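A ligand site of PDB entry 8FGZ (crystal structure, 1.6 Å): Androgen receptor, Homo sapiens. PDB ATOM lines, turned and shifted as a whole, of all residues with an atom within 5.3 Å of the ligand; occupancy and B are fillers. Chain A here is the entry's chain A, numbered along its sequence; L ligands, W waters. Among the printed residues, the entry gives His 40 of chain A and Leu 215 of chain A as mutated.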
ATOM      1  N   HIS A  40     -26.184  11.222 -28.298  1.00  0.00           N
ATOM      2  CA  HIS A  40     -25.644  12.442 -27.715  1.00  0.00           C
ATOM      3  C   HIS A  40     -26.762  13.403 -27.319  1.00  0.00           C
ATOM      4  O   HIS A  40     -26.619  14.153 -26.341  1.00  0.00           O
ATOM      5  CB  HIS A  40     -24.644  13.097 -28.668  1.00  0.00           C
ATOM      6  CG  HIS A  40     -23.296  12.474 -28.593  1.00  0.00           C
ATOM      7  ND1 HIS A  40     -22.320  12.921 -27.735  1.00  0.00           N
ATOM      8  CD2 HIS A  40     -22.756  11.437 -29.280  1.00  0.00           C
ATOM      9  CE1 HIS A  40     -21.246  12.161 -27.871  1.00  0.00           C
ATOM     10  NE2 HIS A  40     -21.479  11.264 -28.811  1.00  0.00           N
ATOM     11  N   LEU A  43     -27.527  12.078 -23.899  1.00  0.00           N
ATOM     12  CA  LEU A  43     -26.460  12.359 -22.953  1.00  0.00           C
ATOM     13  C   LEU A  43     -26.473  13.821 -22.526  1.00  0.00           C
ATOM     14  O   LEU A  43     -26.259  14.150 -21.361  1.00  0.00           O
ATOM     15  CB  LEU A  43     -25.076  11.999 -23.530  1.00  0.00           C
ATOM     16  CG  LEU A  43     -24.718  10.522 -23.628  1.00  0.00           C
ATOM     17  CD1 LEU A  43     -23.558  10.349 -24.606  1.00  0.00           C
ATOM     18  CD2 LEU A  43     -24.398   9.933 -22.245  1.00  0.00           C
ATOM     19  N   ASN A  44     -26.727  14.719 -23.488  1.00  0.00           N
ATOM     20  CA  ASN A  44     -26.716  16.148 -23.176  1.00  0.00           C
ATOM     21  C   ASN A  44     -27.899  16.517 -22.297  1.00  0.00           C
ATOM     22  O   ASN A  44     -27.759  17.323 -21.374  1.00  0.00           O
ATOM     23  CB  ASN A  44     -26.711  16.969 -24.452  1.00  0.00           C
ATOM     24  CG  ASN A  44     -25.364  16.968 -25.121  1.00  0.00           C
ATOM     25  OD1 ASN A  44     -24.335  16.893 -24.445  1.00  0.00           O
ATOM     26  ND2 ASN A  44     -25.340  17.055 -26.440  1.00  0.00           N
ATOM     27  N   LEU A  46     -29.301  14.425 -20.190  1.00  0.00           N
ATOM     28  CA  LEU A  46     -28.964  13.891 -18.872  1.00  0.00           C
ATOM     29  C   LEU A  46     -28.068  14.863 -18.121  1.00  0.00           C
ATOM     30  O   LEU A  46     -28.262  15.123 -16.921  1.00  0.00           O
ATOM     31  CB  LEU A  46     -28.290  12.529 -19.006  1.00  0.00           C
ATOM     32  CG  LEU A  46     -27.844  11.845 -17.703  1.00  0.00           C
ATOM     33  CD1 LEU A  46     -29.077  11.597 -16.797  1.00  0.00           C
ATOM     34  CD2 LEU A  46     -27.108  10.532 -17.959  1.00  0.00           C
ATOM     35  N   GLY A  47     -27.060  15.416 -18.806  1.00  0.00           N
ATOM     36  CA  GLY A  47     -26.189  16.379 -18.150  1.00  0.00           C
ATOM     37  C   GLY A  47     -26.944  17.603 -17.660  1.00  0.00           C
ATOM     38  O   GLY A  47     -26.683  18.119 -16.574  1.00  0.00           O
ATOM     39  N   GLN A  50     -28.788  16.526 -14.545  1.00  0.00           N
ATOM     40  CA  GLN A  50     -27.885  16.344 -13.418  1.00  0.00           C
ATOM     41  C   GLN A  50     -27.320  17.669 -12.933  1.00  0.00           C
ATOM     42  O   GLN A  50     -27.020  17.809 -11.734  1.00  0.00           O
ATOM     43  CB  GLN A  50     -26.760  15.385 -13.820  1.00  0.00           C
ATOM     44  CG  GLN A  50     -27.249  13.956 -14.198  1.00  0.00           C
ATOM     45  CD  GLN A  50     -26.185  12.879 -13.981  1.00  0.00           C
ATOM     46  OE1 GLN A  50     -25.013  13.183 -13.753  1.00  0.00           O
ATOM     47  NE2 GLN A  50     -26.557  11.630 -14.193  1.00  0.00           N
ATOM     48  N   TRP A  80     -18.128  20.049 -12.600  1.00  0.00           N
ATOM     49  CA  TRP A  80     -19.292  19.186 -12.825  1.00  0.00           C
ATOM     50  C   TRP A  80     -18.939  17.921 -13.588  1.00  0.00           C
ATOM     51  O   TRP A  80     -19.498  16.855 -13.317  1.00  0.00           O
ATOM     52  CB  TRP A  80     -20.410  19.951 -13.537  1.00  0.00           C
ATOM     53  CG  TRP A  80     -20.033  20.519 -14.897  1.00  0.00           C
ATOM     54  CD1 TRP A  80     -19.416  21.717 -15.131  1.00  0.00           C
ATOM     55  CD2 TRP A  80     -20.306  19.952 -16.191  1.00  0.00           C
ATOM     56  NE1 TRP A  80     -19.249  21.918 -16.477  1.00  0.00           N
ATOM     57  CE2 TRP A  80     -19.786  20.847 -17.151  1.00  0.00           C
ATOM     58  CE3 TRP A  80     -20.899  18.769 -16.630  1.00  0.00           C
ATOM     59  CZ2 TRP A  80     -19.862  20.607 -18.523  1.00  0.00           C
ATOM     60  CZ3 TRP A  80     -20.981  18.527 -17.995  1.00  0.00           C
ATOM     61  CH2 TRP A  80     -20.464  19.440 -18.924  1.00  0.00           C
ATOM     62  N   MET A  81     -18.016  18.010 -14.564  1.00  0.00           N
ATOM     63  CA  MET A  81     -17.744  16.826 -15.364  1.00  0.00           C
ATOM     64  C   MET A  81     -17.120  15.727 -14.499  1.00  0.00           C
ATOM     65  O   MET A  81     -17.530  14.564 -14.568  1.00  0.00           O
ATOM     66  CB  MET A  81     -16.824  17.164 -16.559  1.00  0.00           C
ATOM     67  CG  MET A  81     -16.515  15.913 -17.400  1.00  0.00           C
ATOM     68  SD  MET A  81     -17.897  15.547 -18.511  1.00  0.00           S
ATOM     69  CE  MET A  81     -17.898  16.986 -19.602  1.00  0.00           C
ATOM     70  N   MET A  84     -19.727  14.239 -12.091  1.00  0.00           N
ATOM     71  CA  MET A  84     -20.725  13.418 -12.763  1.00  0.00           C
ATOM     72  C   MET A  84     -20.118  12.096 -13.240  1.00  0.00           C
ATOM     73  O   MET A  84     -20.763  11.040 -13.157  1.00  0.00           O
ATOM     74  CB  MET A  84     -21.282  14.210 -13.940  1.00  0.00           C
ATOM     75  CG  MET A  84     -22.351  15.233 -13.551  1.00  0.00           C
ATOM     76  SD  MET A  84     -23.063  16.031 -15.008  1.00  0.00           S
ATOM     77  CE  MET A  84     -23.845  17.485 -14.290  1.00  0.00           C
ATOM     78  N   VAL A  85     -18.874  12.139 -13.725  1.00  0.00           N
ATOM     79  CA  VAL A  85     -18.232  10.907 -14.169  1.00  0.00           C
ATOM     80  C   VAL A  85     -17.924  10.010 -12.975  1.00  0.00           C
ATOM     81  O   VAL A  85     -18.092   8.788 -13.034  1.00  0.00           O
ATOM     82  CB  VAL A  85     -16.952  11.235 -14.979  1.00  0.00           C
ATOM     83  CG1 VAL A  85     -16.061  10.007 -15.108  1.00  0.00           C
ATOM     84  CG2 VAL A  85     -17.313  11.854 -16.322  1.00  0.00           C
ATOM     85  N   MET A  88     -21.175   8.434 -11.915  1.00  0.00           N
ATOM     86  CA  MET A  88     -21.592   7.436 -12.887  1.00  0.00           C
ATOM     87  C   MET A  88     -20.754   6.181 -12.753  1.00  0.00           C
ATOM     88  O   MET A  88     -21.252   5.054 -12.919  1.00  0.00           O
ATOM     89  CB  MET A  88     -21.449   8.017 -14.292  1.00  0.00           C
ATOM     90  CG  MET A  88     -21.915   7.146 -15.453  1.00  0.00           C
ATOM     91  SD  MET A  88     -20.737   5.884 -15.970  1.00  0.00           S
ATOM     92  CE  MET A  88     -19.651   6.966 -16.866  1.00  0.00           C
ATOM     93  N   ARG A  91     -22.250   4.225  -9.895  1.00  0.00           N
ATOM     94  CA  ARG A  91     -23.505   3.600 -10.340  1.00  0.00           C
ATOM     95  C   ARG A  91     -23.212   2.376 -11.188  1.00  0.00           C
ATOM     96  O   ARG A  91     -23.889   1.338 -11.073  1.00  0.00           O
ATOM     97  CB  ARG A  91     -24.298   4.602 -11.181  1.00  0.00           C
ATOM     98  CG  ARG A  91     -25.060   5.669 -10.410  1.00  0.00           C
ATOM     99  CD  ARG A  91     -26.157   6.296 -11.272  1.00  0.00           C
ATOM    100  NE  ARG A  91     -25.678   7.025 -12.447  1.00  0.00           N
ATOM    101  CZ  ARG A  91     -25.049   8.192 -12.454  1.00  0.00           C
ATOM    102  NH1 ARG A  91     -24.760   8.832 -11.319  1.00  0.00           N
ATOM    103  NH2 ARG A  91     -24.732   8.762 -13.619  1.00  0.00           N
ATOM    104  N   PHE A 103     -25.165   5.257 -17.294  1.00  0.00           N
ATOM    105  CA  PHE A 103     -25.324   6.701 -17.246  1.00  0.00           C
ATOM    106  C   PHE A 103     -26.634   7.042 -16.549  1.00  0.00           C
ATOM    107  O   PHE A 103     -26.706   7.953 -15.734  1.00  0.00           O
ATOM    108  CB  PHE A 103     -25.327   7.302 -18.653  1.00  0.00           C
ATOM    109  CG  PHE A 103     -23.978   7.266 -19.331  1.00  0.00           C
ATOM    110  CD1 PHE A 103     -22.997   8.174 -19.010  1.00  0.00           C
ATOM    111  CD2 PHE A 103     -23.740   6.345 -20.331  1.00  0.00           C
ATOM    112  CE1 PHE A 103     -21.781   8.132 -19.631  1.00  0.00           C
ATOM    113  CE2 PHE A 103     -22.514   6.309 -20.983  1.00  0.00           C
ATOM    114  CZ  PHE A 103     -21.526   7.214 -20.628  1.00  0.00           C
ATOM    115  N   MET A 119     -17.458   7.773 -28.885  1.00  0.00           N
ATOM    116  CA  MET A 119     -16.734   8.011 -27.626  1.00  0.00           C
ATOM    117  C   MET A 119     -16.096   6.746 -27.065  1.00  0.00           C
ATOM    118  O   MET A 119     -15.933   6.629 -25.848  1.00  0.00           O
ATOM    119  CB  MET A 119     -17.661   8.587 -26.545  1.00  0.00           C
ATOM    120  CG  MET A 119     -18.432   9.855 -26.865  1.00  0.00           C
ATOM    121  SD  MET A 119     -19.661  10.093 -25.554  1.00  0.00           S
ATOM    122  CE  MET A 119     -18.573  10.029 -24.150  1.00  0.00           C
ATOM    123  N   MET A 126     -13.572   5.506 -18.752  1.00  0.00           N
ATOM    124  CA  MET A 126     -14.614   5.583 -17.723  1.00  0.00           C
ATOM    125  C   MET A 126     -14.919   4.215 -17.129  1.00  0.00           C
ATOM    126  O   MET A 126     -15.217   4.097 -15.933  1.00  0.00           O
ATOM    127  CB  MET A 126     -15.873   6.238 -18.305  1.00  0.00           C
ATOM    128  CG  MET A 126     -15.732   7.777 -18.397  1.00  0.00           C
ATOM    129  SD  MET A 126     -17.232   8.619 -18.964  1.00  0.00           S
ATOM    130  CE  MET A 126     -17.304   8.203 -20.709  1.00  0.00           C
ATOM    131  N   LEU A 212     -13.182  14.482 -21.702  1.00  0.00           N
ATOM    132  CA  LEU A 212     -14.588  14.687 -21.988  1.00  0.00           C
ATOM    133  C   LEU A 212     -14.898  16.166 -22.208  1.00  0.00           C
ATOM    134  O   LEU A 212     -15.742  16.508 -23.035  1.00  0.00           O
ATOM    135  CB  LEU A 212     -15.476  14.116 -20.863  1.00  0.00           C
ATOM    136  CG  LEU A 212     -15.398  12.586 -20.817  1.00  0.00           C
ATOM    137  CD1 LEU A 212     -15.651  12.018 -19.412  1.00  0.00           C
ATOM    138  CD2 LEU A 212     -16.240  11.940 -21.907  1.00  0.00           C
ATOM    139  N   LEU A 215     -13.987  16.787 -25.753  1.00  0.00           N
ATOM    140  CA  LEU A 215     -14.988  16.207 -26.633  1.00  0.00           C
ATOM    141  C   LEU A 215     -16.246  17.067 -26.706  1.00  0.00           C
ATOM    142  O   LEU A 215     -16.759  17.349 -27.791  1.00  0.00           O
ATOM    143  CB  LEU A 215     -15.315  14.795 -26.145  1.00  0.00           C
ATOM    144  CG  LEU A 215     -16.437  14.086 -26.883  1.00  0.00           C
ATOM    145  CD1 LEU A 215     -15.985  13.655 -28.274  1.00  0.00           C
ATOM    146  CD2 LEU A 215     -16.892  12.859 -26.078  1.00  0.00           C
ATOM    147  N   THR A 216     -16.783  17.448 -25.549  1.00  0.00           N
ATOM    148  CA  THR A 216     -18.054  18.175 -25.563  1.00  0.00           C
ATOM    149  C   THR A 216     -17.916  19.561 -26.179  1.00  0.00           C
ATOM    150  O   THR A 216     -18.835  20.025 -26.870  1.00  0.00           O
ATOM    151  CB  THR A 216     -18.661  18.214 -24.143  1.00  0.00           C
ATOM    152  OG1 THR A 216     -20.059  18.480 -24.249  1.00  0.00           O
ATOM    153  CG2 THR A 216     -17.994  19.274 -23.254  1.00  0.00           C
ATOM    154  N   LEU A 219     -17.913  18.966 -29.933  1.00  0.00           N
ATOM    155  CA  LEU A 219     -19.253  18.629 -30.382  1.00  0.00           C
ATOM    156  C   LEU A 219     -20.186  19.836 -30.340  1.00  0.00           C
ATOM    157  O   LEU A 219     -21.043  19.985 -31.225  1.00  0.00           O
ATOM    158  CB  LEU A 219     -19.802  17.473 -29.558  1.00  0.00           C
ATOM    159  CG  LEU A 219     -18.968  16.190 -29.631  1.00  0.00           C
ATOM    160  CD1 LEU A 219     -19.719  15.060 -28.957  1.00  0.00           C
ATOM    161  CD2 LEU A 219     -18.798  15.839 -31.104  1.00  0.00           C
ATOM    162  N   PHE A 230     -27.524  22.502 -28.113  1.00  0.00           N
ATOM    163  CA  PHE A 230     -27.399  21.811 -26.843  1.00  0.00           C
ATOM    164  C   PHE A 230     -28.477  22.348 -25.899  1.00  0.00           C
ATOM    165  O   PHE A 230     -29.041  23.419 -26.145  1.00  0.00           O
ATOM    166  CB  PHE A 230     -26.025  22.082 -26.258  1.00  0.00           C
ATOM    167  CG  PHE A 230     -24.951  21.113 -26.668  1.00  0.00           C
ATOM    168  CD1 PHE A 230     -24.793  20.715 -28.000  1.00  0.00           C
ATOM    169  CD2 PHE A 230     -24.028  20.652 -25.735  1.00  0.00           C
ATOM    170  CE1 PHE A 230     -23.772  19.852 -28.357  1.00  0.00           C
ATOM    171  CE2 PHE A 230     -23.014  19.796 -26.096  1.00  0.00           C
ATOM    172  CZ  PHE A 230     -22.876  19.391 -27.406  1.00  0.00           C
ATOM    173  N   MET A 234     -26.175  23.684 -20.471  1.00  0.00           N
ATOM    174  CA  MET A 234     -24.970  23.046 -20.993  1.00  0.00           C
ATOM    175  C   MET A 234     -24.305  23.930 -22.032  1.00  0.00           C
ATOM    176  O   MET A 234     -23.083  24.087 -22.014  1.00  0.00           O
ATOM    177  CB  MET A 234     -25.274  21.667 -21.589  1.00  0.00           C
ATOM    178  CG  MET A 234     -25.777  20.625 -20.589  1.00  0.00           C
ATOM    179  SD  MET A 234     -24.408  19.836 -19.708  1.00  0.00           S
ATOM    180  CE  MET A 234     -23.839  18.672 -20.953  1.00  0.00           C
ATOM    181  N   ILE A 238     -20.536  25.244 -21.523  1.00  0.00           N
ATOM    182  CA  ILE A 238     -19.514  24.686 -22.385  1.00  0.00           C
ATOM    183  C   ILE A 238     -18.885  25.760 -23.244  1.00  0.00           C
ATOM    184  O   ILE A 238     -17.728  25.626 -23.670  1.00  0.00           O
ATOM    185  CB  ILE A 238     -20.080  23.542 -23.247  1.00  0.00           C
ATOM    186  CG1 ILE A 238     -20.458  22.376 -22.323  1.00  0.00           C
ATOM    187  CG2 ILE A 238     -19.029  23.065 -24.253  1.00  0.00           C
ATOM    188  CD1 ILE A 238     -21.299  21.292 -23.017  1.00  0.00           C
HETATM  189  C1  LIG L   1     -23.872  12.934 -18.304  1.00  0.00           C
HETATM  190  C2  LIG L   1     -24.043  12.438 -16.870  1.00  0.00           C
HETATM  191  C3  LIG L   1     -23.224  11.219 -16.575  1.00  0.00           C
HETATM  192  O1  LIG L   1     -23.678  10.270 -15.976  1.00  0.00           O
HETATM  193  C4  LIG L   1     -21.811  11.256 -17.073  1.00  0.00           C
HETATM  194  C5  LIG L   1     -21.773  11.670 -18.543  1.00  0.00           C
HETATM  195  C6  LIG L   1     -20.329  11.715 -19.053  1.00  0.00           C
HETATM  196  C7  LIG L   1     -20.286  12.079 -20.533  1.00  0.00           C
HETATM  197  C8  LIG L   1     -20.903  13.453 -20.790  1.00  0.00           C
HETATM  198  C9  LIG L   1     -22.345  13.442 -20.255  1.00  0.00           C
HETATM  199  C10 LIG L   1     -22.408  13.071 -18.752  1.00  0.00           C
HETATM  200  C11 LIG L   1     -23.027  14.785 -20.552  1.00  0.00           C
HETATM  201  C12 LIG L   1     -23.014  15.129 -22.040  1.00  0.00           C
HETATM  202  C13 LIG L   1     -21.598  15.076 -22.633  1.00  0.00           C
HETATM  203  C14 LIG L   1     -21.004  13.696 -22.301  1.00  0.00           C
HETATM  204  C15 LIG L   1     -19.696  13.711 -23.127  1.00  0.00           C
HETATM  205  C16 LIG L   1     -20.068  14.509 -24.396  1.00  0.00           C
HETATM  206  C17 LIG L   1     -21.497  15.029 -24.159  1.00  0.00           C
HETATM  207  O2  LIG L   1     -21.653  16.332 -24.725  1.00  0.00           O
HETATM  208  C18 LIG L   1     -20.750  16.243 -22.089  1.00  0.00           C
HETATM  209  C19 LIG L   1     -21.728  14.136 -17.878  1.00  0.00           C
HETATM  210  O   HOH W   1     -22.502  15.741 -27.353  1.00  0.00           O
HETATM  211  O   HOH W   2     -23.599  11.255 -12.750  1.00  0.00           O
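Water W1 lies within hydrogen-bond range of O2 of the ligand (2.8 Å), ND1 of His 40 (2.9 Å) and ND2 of Asn 44 (3.3 Å).
O2 of the ligand lies within hydrogen-bond range of OD1 of Asn 44 (2.8 Å). An oxygen (O1) of the ligand is in hydrogen-bond range of the guanidinium group (NH2) of Arg 91 (3.0 Å). The side-chain hydroxyl (OG1) of Thr 216 sits at hydrogen-bond distance from an oxygen (O2) of the ligand (2.7 Å).
The side-chain amide nitrogen of Gln 50 lies close to the guanidinium group of Arg 91. The side-chain amide nitrogen (ND2) of Asn 44 lies within hydrogen-bond range of the backbone carbonyl oxygen (O) of His 40 (3.2 Å). OE1 of Gln 50 lies close to SD of Met 84, 3.7 Å away. The guanidinium group of Arg 91 sits at hydrogen-bond distance from the backbone carbonyl oxygen of Phe 103 (3.0 Å).
Leu 43 touches the ligand. CD2 of Leu 46 touches C2 of the ligand (3.8 Å). Gln 50 touches the ligand (OE1 to C2, 3.3 Å). Met 81 touches the ligand (CE to C18, 3.9 Å). SD of Met 84 touches C19 of the ligand, 3.7 Å away. Met 88 touches the ligand. Phe 103 touches the ligand. Met 119 touches the ligand (CE to C15, 3.98 Å). Leu 215 touches the ligand. Phe 230 touches the ligand (CE2 to O2, 3.97 Å). CE of Met 234 touches C12 of the ligand (3.8 Å). Hydrophobic or aromatic side chains that line the ligand: Leu 46, Met 81, Met 84, Met 88, Phe 103, Met 119, Leu 215, Phe 230 and Met 234. Of the 22 residues printed, 14 come within 4 Å of the ligand.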
